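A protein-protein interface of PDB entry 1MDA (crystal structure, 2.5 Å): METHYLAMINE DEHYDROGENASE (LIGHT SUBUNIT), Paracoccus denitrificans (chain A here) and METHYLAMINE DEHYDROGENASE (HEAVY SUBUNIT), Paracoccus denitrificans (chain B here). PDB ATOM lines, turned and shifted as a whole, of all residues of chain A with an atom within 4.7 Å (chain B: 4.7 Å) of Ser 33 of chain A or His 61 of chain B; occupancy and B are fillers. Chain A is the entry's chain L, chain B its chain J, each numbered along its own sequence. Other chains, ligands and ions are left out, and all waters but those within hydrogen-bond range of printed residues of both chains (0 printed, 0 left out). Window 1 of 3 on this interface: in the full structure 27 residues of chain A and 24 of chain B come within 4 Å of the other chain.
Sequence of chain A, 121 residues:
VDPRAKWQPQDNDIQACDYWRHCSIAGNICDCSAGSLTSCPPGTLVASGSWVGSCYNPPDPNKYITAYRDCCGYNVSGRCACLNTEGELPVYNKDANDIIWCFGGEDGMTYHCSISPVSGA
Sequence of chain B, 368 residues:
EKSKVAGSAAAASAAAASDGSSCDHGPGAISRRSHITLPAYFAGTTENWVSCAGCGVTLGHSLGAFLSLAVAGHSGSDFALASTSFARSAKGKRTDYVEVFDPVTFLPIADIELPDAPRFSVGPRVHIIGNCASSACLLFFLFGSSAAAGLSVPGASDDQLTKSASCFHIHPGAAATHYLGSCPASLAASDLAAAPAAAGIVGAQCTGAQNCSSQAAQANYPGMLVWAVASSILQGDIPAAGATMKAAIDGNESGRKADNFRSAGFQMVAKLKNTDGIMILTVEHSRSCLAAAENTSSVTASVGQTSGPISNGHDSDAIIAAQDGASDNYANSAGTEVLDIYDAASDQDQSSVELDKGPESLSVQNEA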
ATOM      1  N   ILE A  29     -19.964  -0.236   2.312  1.00  0.00           N
ATOM      2  CA  ILE A  29     -21.223  -0.049   1.660  1.00  0.00           C
ATOM      3  C   ILE A  29     -21.036   0.211   0.141  1.00  0.00           C
ATOM      4  O   ILE A  29     -20.212   1.054  -0.236  1.00  0.00           O
ATOM      5  CB  ILE A  29     -21.939   1.063   2.411  1.00  0.00           C
ATOM      6  CG1 ILE A  29     -22.058   0.701   3.902  1.00  0.00           C
ATOM      7  CG2 ILE A  29     -23.322   1.277   1.812  1.00  0.00           C
ATOM      8  CD1 ILE A  29     -22.800   1.750   4.757  1.00  0.00           C
ATOM      9  N   CYS A  30     -21.768  -0.521  -0.748  1.00  0.00           N
ATOM     10  CA  CYS A  30     -21.664  -0.394  -2.235  1.00  0.00           C
ATOM     11  C   CYS A  30     -22.115   0.923  -2.824  1.00  0.00           C
ATOM     12  O   CYS A  30     -21.674   1.330  -3.870  1.00  0.00           O
ATOM     13  CB  CYS A  30     -22.181  -1.576  -3.125  1.00  0.00           C
ATOM     14  SG  CYS A  30     -21.416  -3.054  -2.462  1.00  0.00           S
ATOM     15  N   ASP A  31     -23.052   1.559  -2.187  1.00  0.00           N
ATOM     16  CA  ASP A  31     -23.615   2.765  -2.730  1.00  0.00           C
ATOM     17  C   ASP A  31     -22.558   3.865  -2.815  1.00  0.00           C
ATOM     18  O   ASP A  31     -22.636   4.818  -3.603  1.00  0.00           O
ATOM     19  CB  ASP A  31     -24.773   3.132  -1.803  1.00  0.00           C
ATOM     20  CG  ASP A  31     -25.790   4.029  -2.399  1.00  0.00           C
ATOM     21  OD1 ASP A  31     -26.190   3.921  -3.537  1.00  0.00           O
ATOM     22  OD2 ASP A  31     -26.126   4.965  -1.571  1.00  0.00           O
ATOM     23  N   CYS A  32     -21.533   3.695  -1.997  1.00  0.00           N
ATOM     24  CA  CYS A  32     -20.416   4.617  -1.877  1.00  0.00           C
ATOM     25  C   CYS A  32     -19.316   4.448  -2.928  1.00  0.00           C
ATOM     26  O   CYS A  32     -18.422   5.292  -3.029  1.00  0.00           O
ATOM     27  CB  CYS A  32     -19.823   4.497  -0.463  1.00  0.00           C
ATOM     28  SG  CYS A  32     -21.031   4.698   0.856  1.00  0.00           S
ATOM     29  N   SER A  33     -19.388   3.380  -3.727  1.00  0.00           N
ATOM     30  CA  SER A  33     -18.388   3.107  -4.761  1.00  0.00           C
ATOM     31  C   SER A  33     -19.023   2.795  -6.117  1.00  0.00           C
ATOM     32  O   SER A  33     -18.393   2.111  -6.932  1.00  0.00           O
ATOM     33  CB  SER A  33     -17.395   1.996  -4.378  1.00  0.00           C
ATOM     34  OG  SER A  33     -18.003   0.731  -4.472  1.00  0.00           O
ATOM     35  N   ALA A  34     -20.260   3.330  -6.310  1.00  0.00           N
ATOM     36  CA  ALA A  34     -21.088   3.241  -7.495  1.00  0.00           C
ATOM     37  C   ALA A  34     -22.113   2.110  -7.567  1.00  0.00           C
ATOM     38  O   ALA A  34     -22.720   1.835  -8.603  1.00  0.00           O
ATOM     39  CB  ALA A  34     -20.196   3.133  -8.685  1.00  0.00           C
ATOM     40  N   GLY A  35     -22.231   1.341  -6.527  1.00  0.00           N
ATOM     41  CA  GLY A  35     -23.232   0.323  -6.573  1.00  0.00           C
ATOM     42  C   GLY A  35     -24.506   1.013  -6.154  1.00  0.00           C
ATOM     43  O   GLY A  35     -24.667   2.214  -6.357  1.00  0.00           O
ATOM     44  N   PRO A  41     -21.421  -2.319  -8.019  1.00  0.00           N
ATOM     45  CA  PRO A  41     -20.891  -1.347  -8.930  1.00  0.00           C
ATOM     46  C   PRO A  41     -20.494  -2.088 -10.200  1.00  0.00           C
ATOM     47  O   PRO A  41     -20.326  -3.310 -10.177  1.00  0.00           O
ATOM     48  CB  PRO A  41     -19.664  -0.730  -8.220  1.00  0.00           C
ATOM     49  CG  PRO A  41     -19.617  -1.292  -6.809  1.00  0.00           C
ATOM     50  CD  PRO A  41     -20.603  -2.453  -6.783  1.00  0.00           C
ATOM     51  N   TYR A  74     -12.421  -6.806  -7.353  1.00  0.00           N
ATOM     52  CA  TYR A  74     -11.858  -5.479  -7.150  1.00  0.00           C
ATOM     53  C   TYR A  74     -11.246  -5.425  -5.764  1.00  0.00           C
ATOM     54  O   TYR A  74     -11.371  -6.353  -4.971  1.00  0.00           O
ATOM     55  CB  TYR A  74     -12.882  -4.323  -7.238  1.00  0.00           C
ATOM     56  CG  TYR A  74     -13.077  -3.618  -8.571  1.00  0.00           C
ATOM     57  CD1 TYR A  74     -13.340  -4.327  -9.740  1.00  0.00           C
ATOM     58  CD2 TYR A  74     -13.253  -2.232  -8.599  1.00  0.00           C
ATOM     59  CE1 TYR A  74     -13.608  -3.667 -10.939  1.00  0.00           C
ATOM     60  CE2 TYR A  74     -13.543  -1.554  -9.778  1.00  0.00           C
ATOM     61  CZ  TYR A  74     -13.704  -2.280 -10.959  1.00  0.00           C
ATOM     62  OH  TYR A  74     -13.974  -1.649 -12.136  1.00  0.00           O
ATOM     63  N   SER A  77     -12.955  -0.796  -1.577  1.00  0.00           N
ATOM     64  CA  SER A  77     -13.322   0.519  -2.022  1.00  0.00           C
ATOM     65  C   SER A  77     -12.722   1.616  -1.149  1.00  0.00           C
ATOM     66  O   SER A  77     -12.377   2.695  -1.634  1.00  0.00           O
ATOM     67  CB  SER A  77     -14.824   0.665  -2.060  1.00  0.00           C
ATOM     68  OG  SER A  77     -15.293   1.115  -0.818  1.00  0.00           O
ATOM     69  N   ARG A  79     -14.282   3.271   0.966  1.00  0.00           N
ATOM     70  CA  ARG A  79     -15.312   4.265   1.205  1.00  0.00           C
ATOM     71  C   ARG A  79     -16.053   4.192   2.527  1.00  0.00           C
ATOM     72  O   ARG A  79     -15.516   4.494   3.593  1.00  0.00           O
ATOM     73  CB  ARG A  79     -16.118   4.725   0.000  1.00  0.00           C
ATOM     74  CG  ARG A  79     -15.148   5.047  -1.121  1.00  0.00           C
ATOM     75  CD  ARG A  79     -15.557   6.124  -2.120  1.00  0.00           C
ATOM     76  NE  ARG A  79     -15.674   7.475  -1.540  1.00  0.00           N
ATOM     77  CZ  ARG A  79     -16.846   8.076  -1.270  1.00  0.00           C
ATOM     78  NH1 ARG A  79     -18.020   7.489  -1.527  1.00  0.00           N
ATOM     79  NH2 ARG A  79     -16.849   9.314  -0.790  1.00  0.00           N
ATOM     80  N   HIS A 112     -14.466  -6.253  -2.377  1.00  0.00           N
ATOM     81  CA  HIS A 112     -14.621  -4.849  -2.755  1.00  0.00           C
ATOM     82  C   HIS A 112     -15.721  -4.196  -1.988  1.00  0.00           C
ATOM     83  O   HIS A 112     -15.578  -3.114  -1.443  1.00  0.00           O
ATOM     84  CB  HIS A 112     -14.967  -4.597  -4.239  1.00  0.00           C
ATOM     85  CG  HIS A 112     -15.223  -3.150  -4.592  1.00  0.00           C
ATOM     86  ND1 HIS A 112     -14.178  -2.230  -4.763  1.00  0.00           N
ATOM     87  CD2 HIS A 112     -16.387  -2.501  -4.916  1.00  0.00           C
ATOM     88  CE1 HIS A 112     -14.720  -1.066  -5.130  1.00  0.00           C
ATOM     89  NE2 HIS A 112     -16.048  -1.190  -5.225  1.00  0.00           N
ATOM     90  N   CYS A 113     -16.792  -4.968  -1.923  1.00  0.00           N
ATOM     91  CA  CYS A 113     -18.064  -4.472  -1.537  1.00  0.00           C
ATOM     92  C   CYS A 113     -19.013  -5.451  -0.853  1.00  0.00           C
ATOM     93  O   CYS A 113     -19.036  -6.644  -1.152  1.00  0.00           O
ATOM     94  CB  CYS A 113     -18.632  -4.145  -2.949  1.00  0.00           C
ATOM     95  SG  CYS A 113     -19.426  -2.623  -2.594  1.00  0.00           S
ATOM     96  N   GLU B  47      -5.661   3.154  -7.268  1.00  0.00           N
ATOM     97  CA  GLU B  47      -7.051   3.282  -7.634  1.00  0.00           C
ATOM     98  C   GLU B  47      -7.363   4.543  -8.458  1.00  0.00           C
ATOM     99  O   GLU B  47      -6.748   5.613  -8.300  1.00  0.00           O
ATOM    100  CB  GLU B  47      -7.891   3.264  -6.347  1.00  0.00           C
ATOM    101  CG  GLU B  47      -7.854   1.914  -5.612  1.00  0.00           C
ATOM    102  CD  GLU B  47      -8.540   1.917  -4.264  1.00  0.00           C
ATOM    103  OE1 GLU B  47      -7.958   2.687  -3.398  1.00  0.00           O
ATOM    104  OE2 GLU B  47      -9.461   1.177  -3.982  1.00  0.00           O
ATOM    105  N   ASN B  48      -8.428   4.430  -9.265  1.00  0.00           N
ATOM    106  CA  ASN B  48      -8.933   5.496 -10.131  1.00  0.00           C
ATOM    107  C   ASN B  48     -10.430   5.630  -9.906  1.00  0.00           C
ATOM    108  O   ASN B  48     -11.199   4.660  -9.881  1.00  0.00           O
ATOM    109  CB  ASN B  48      -8.647   5.201 -11.629  1.00  0.00           C
ATOM    110  CG  ASN B  48      -9.090   6.227 -12.691  1.00  0.00           C
ATOM    111  OD1 ASN B  48      -9.245   5.902 -13.892  1.00  0.00           O
ATOM    112  ND2 ASN B  48      -9.108   7.501 -12.321  1.00  0.00           N
ATOM    113  N   TRP B  49     -10.818   6.856  -9.613  1.00  0.00           N
ATOM    114  CA  TRP B  49     -12.195   7.203  -9.380  1.00  0.00           C
ATOM    115  C   TRP B  49     -12.888   7.851 -10.558  1.00  0.00           C
ATOM    116  O   TRP B  49     -12.368   8.779 -11.187  1.00  0.00           O
ATOM    117  CB  TRP B  49     -12.350   8.064  -8.133  1.00  0.00           C
ATOM    118  CG  TRP B  49     -12.377   7.261  -6.894  1.00  0.00           C
ATOM    119  CD1 TRP B  49     -13.499   6.827  -6.275  1.00  0.00           C
ATOM    120  CD2 TRP B  49     -11.277   6.853  -6.092  1.00  0.00           C
ATOM    121  NE1 TRP B  49     -13.170   6.133  -5.151  1.00  0.00           N
ATOM    122  CE2 TRP B  49     -11.813   6.137  -5.005  1.00  0.00           C
ATOM    123  CE3 TRP B  49      -9.910   7.010  -6.196  1.00  0.00           C
ATOM    124  CZ2 TRP B  49     -11.008   5.551  -4.064  1.00  0.00           C
ATOM    125  CZ3 TRP B  49      -9.111   6.413  -5.261  1.00  0.00           C
ATOM    126  CH2 TRP B  49      -9.656   5.718  -4.193  1.00  0.00           C
ATOM    127  N   VAL B  50     -14.070   7.339 -10.824  1.00  0.00           N
ATOM    128  CA  VAL B  50     -14.934   7.871 -11.840  1.00  0.00           C
ATOM    129  C   VAL B  50     -16.094   8.503 -11.093  1.00  0.00           C
ATOM    130  O   VAL B  50     -16.859   7.782 -10.437  1.00  0.00           O
ATOM    131  CB  VAL B  50     -15.384   6.735 -12.716  1.00  0.00           C
ATOM    132  CG1 VAL B  50     -15.436   7.184 -14.165  1.00  0.00           C
ATOM    133  CG2 VAL B  50     -14.397   5.585 -12.549  1.00  0.00           C
ATOM    134  N   THR B  58     -19.725   9.010  -7.337  1.00  0.00           N
ATOM    135  CA  THR B  58     -18.758   8.110  -7.956  1.00  0.00           C
ATOM    136  C   THR B  58     -19.582   7.092  -8.772  1.00  0.00           C
ATOM    137  O   THR B  58     -20.543   6.539  -8.252  1.00  0.00           O
ATOM    138  CB  THR B  58     -18.013   7.325  -6.848  1.00  0.00           C
ATOM    139  OG1 THR B  58     -17.235   8.163  -6.035  1.00  0.00           O
ATOM    140  CG2 THR B  58     -17.190   6.158  -7.396  1.00  0.00           C
ATOM    141  N   GLY B  60     -18.093   4.603 -10.559  1.00  0.00           N
ATOM    142  CA  GLY B  60     -17.285   3.416 -10.642  1.00  0.00           C
ATOM    143  C   GLY B  60     -15.904   3.677 -10.060  1.00  0.00           C
ATOM    144  O   GLY B  60     -15.640   4.720  -9.452  1.00  0.00           O
ATOM    145  N   HIS B  61     -15.018   2.739 -10.335  1.00  0.00           N
ATOM    146  CA  HIS B  61     -13.684   2.736  -9.801  1.00  0.00           C
ATOM    147  C   HIS B  61     -12.925   1.778 -10.758  1.00  0.00           C
ATOM    148  O   HIS B  61     -13.532   0.964 -11.429  1.00  0.00           O
ATOM    149  CB  HIS B  61     -13.964   2.030  -8.443  1.00  0.00           C
ATOM    150  CG  HIS B  61     -13.476   2.452  -7.086  1.00  0.00           C
ATOM    151  ND1 HIS B  61     -14.403   2.752  -6.119  1.00  0.00           N
ATOM    152  CD2 HIS B  61     -12.263   2.363  -6.455  1.00  0.00           C
ATOM    153  CE1 HIS B  61     -13.768   2.903  -4.971  1.00  0.00           C
ATOM    154  NE2 HIS B  61     -12.468   2.699  -5.136  1.00  0.00           N
ATOM    155  N   SER B  62     -11.607   1.858 -10.816  1.00  0.00           N
ATOM    156  CA  SER B  62     -10.756   1.000 -11.614  1.00  0.00           C
ATOM    157  C   SER B  62      -9.529   0.725 -10.784  1.00  0.00           C
ATOM    158  O   SER B  62      -9.101   1.550  -9.989  1.00  0.00           O
ATOM    159  CB  SER B  62     -10.222   1.601 -12.943  1.00  0.00           C
ATOM    160  OG  SER B  62     -11.269   1.712 -13.921  1.00  0.00           O
ATOM    161  N   LEU B  63      -9.030  -0.468 -10.883  1.00  0.00           N
ATOM    162  CA  LEU B  63      -7.848  -0.804 -10.157  1.00  0.00           C
ATOM    163  C   LEU B  63      -6.631  -0.817 -11.060  1.00  0.00           C
ATOM    164  O   LEU B  63      -6.685  -1.273 -12.191  1.00  0.00           O
ATOM    165  CB  LEU B  63      -8.015  -2.114  -9.369  1.00  0.00           C
ATOM    166  CG  LEU B  63      -8.673  -1.893  -8.037  1.00  0.00           C
ATOM    167  CD1 LEU B  63      -9.346  -3.179  -7.685  1.00  0.00           C
ATOM    168  CD2 LEU B  63      -7.597  -1.494  -6.997  1.00  0.00           C
ATOM    169  N   PHE B 106     -17.079  -0.869 -17.505  1.00  0.00           N
ATOM    170  CA  PHE B 106     -15.832  -0.893 -16.768  1.00  0.00           C
ATOM    171  C   PHE B 106     -15.041  -2.180 -16.944  1.00  0.00           C
ATOM    172  O   PHE B 106     -14.118  -2.459 -16.162  1.00  0.00           O
ATOM    173  CB  PHE B 106     -16.097  -0.626 -15.279  1.00  0.00           C
ATOM    174  CG  PHE B 106     -16.466   0.801 -15.009  1.00  0.00           C
ATOM    175  CD1 PHE B 106     -17.217   1.528 -15.930  1.00  0.00           C
ATOM    176  CD2 PHE B 106     -15.926   1.469 -13.915  1.00  0.00           C
ATOM    177  CE1 PHE B 106     -17.518   2.871 -15.709  1.00  0.00           C
ATOM    178  CE2 PHE B 106     -16.215   2.809 -13.666  1.00  0.00           C
ATOM    179  CZ  PHE B 106     -17.006   3.509 -14.577  1.00  0.00           C
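Hydrophobic or aromatic side chains of chain A within 4 Å of the printed part of chain B: Ala 34, Tyr 74 and His 112.
Of chain B, only His 61 (3.5 Å) comes within 4 Å of Ser 33 of chain A. Of the printed residues of chain B, Ser 77 of chain A touches Trp 49 (3.99 Å) and His 61 (3.5 Å). Printed residues of chain B within 4 Å of His 112 of chain A: His 61 (3.96 Å). Printed residues of chain A within 4 Å of Phe 106 of chain B: Tyr 74. Of the printed residues of chain A, Gly 60 of chain B touches Ala 34. Of the printed residues of chain B, Tyr 74 of chain A touches His 61 (2.7 Å), Leu 63 (3.4 Å) and Phe 106 (3.9 Å). Cys 30 of chain A touches none of the printed residues of chain B. The nearest printed residue of chain A that does not touch Trp 49 of chain B is Cys 32 of chain A (5.7 Å).
N of Val 50 of chain B sits at hydrogen-bond distance from O of Gly 60 of chain B, 3.3 Å away. The side-chain hydroxyl (OG) of Ser 77 of chain A lies within hydrogen-bond range of the backbone NH (N) of Arg 79 of chain A (3.0 Å). The backbone carbonyl oxygen of Cys 32 of chain A sits at hydrogen-bond distance from the guanidinium group of Arg 79 of chain A, at 2.7 Å. The side-chain hydroxyl of Ser 33 of chain A is in hydrogen-bond range of a ring nitrogen (NE2) of His 112 of chain A (2.8 Å). The side-chain sulfur (SG) of Cys 113 of chain A forms a disulfide with the side-chain sulfur (SG) of Cys 30 of chain A, at 2.0 Å.
ND1 of His 61 of chain B touches CB of Ser 33 of chain A, 3.5 Å away. Ala 34 of chain A touches Thr 58 of chain B (CA to O, 3.4 Å). N of Gly 60 of chain B touches CB of Ala 34 of chain A (3.2 Å). Tyr 74 of chain A touches Leu 63 of chain B (CA to CD1, 3.4 Å). Tyr 74 of chain A touches Phe 106 of chain B. Ser 77 of chain A touches Trp 49 of chain B. His 61 of chain B touches Ser 77 of chain A (NE2 to O, 3.5 Å). CD of Arg 79 of chain A touches NE1 of Trp 49 of chain B, at 3.9 Å. His 61 of chain B touches His 112 of chain A.
The side-chain hydroxyl (OH) of Tyr 74 of chain A sits at hydrogen-bond distance from the backbone carbonyl oxygen (O) of His 61 of chain B (2.7 Å).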
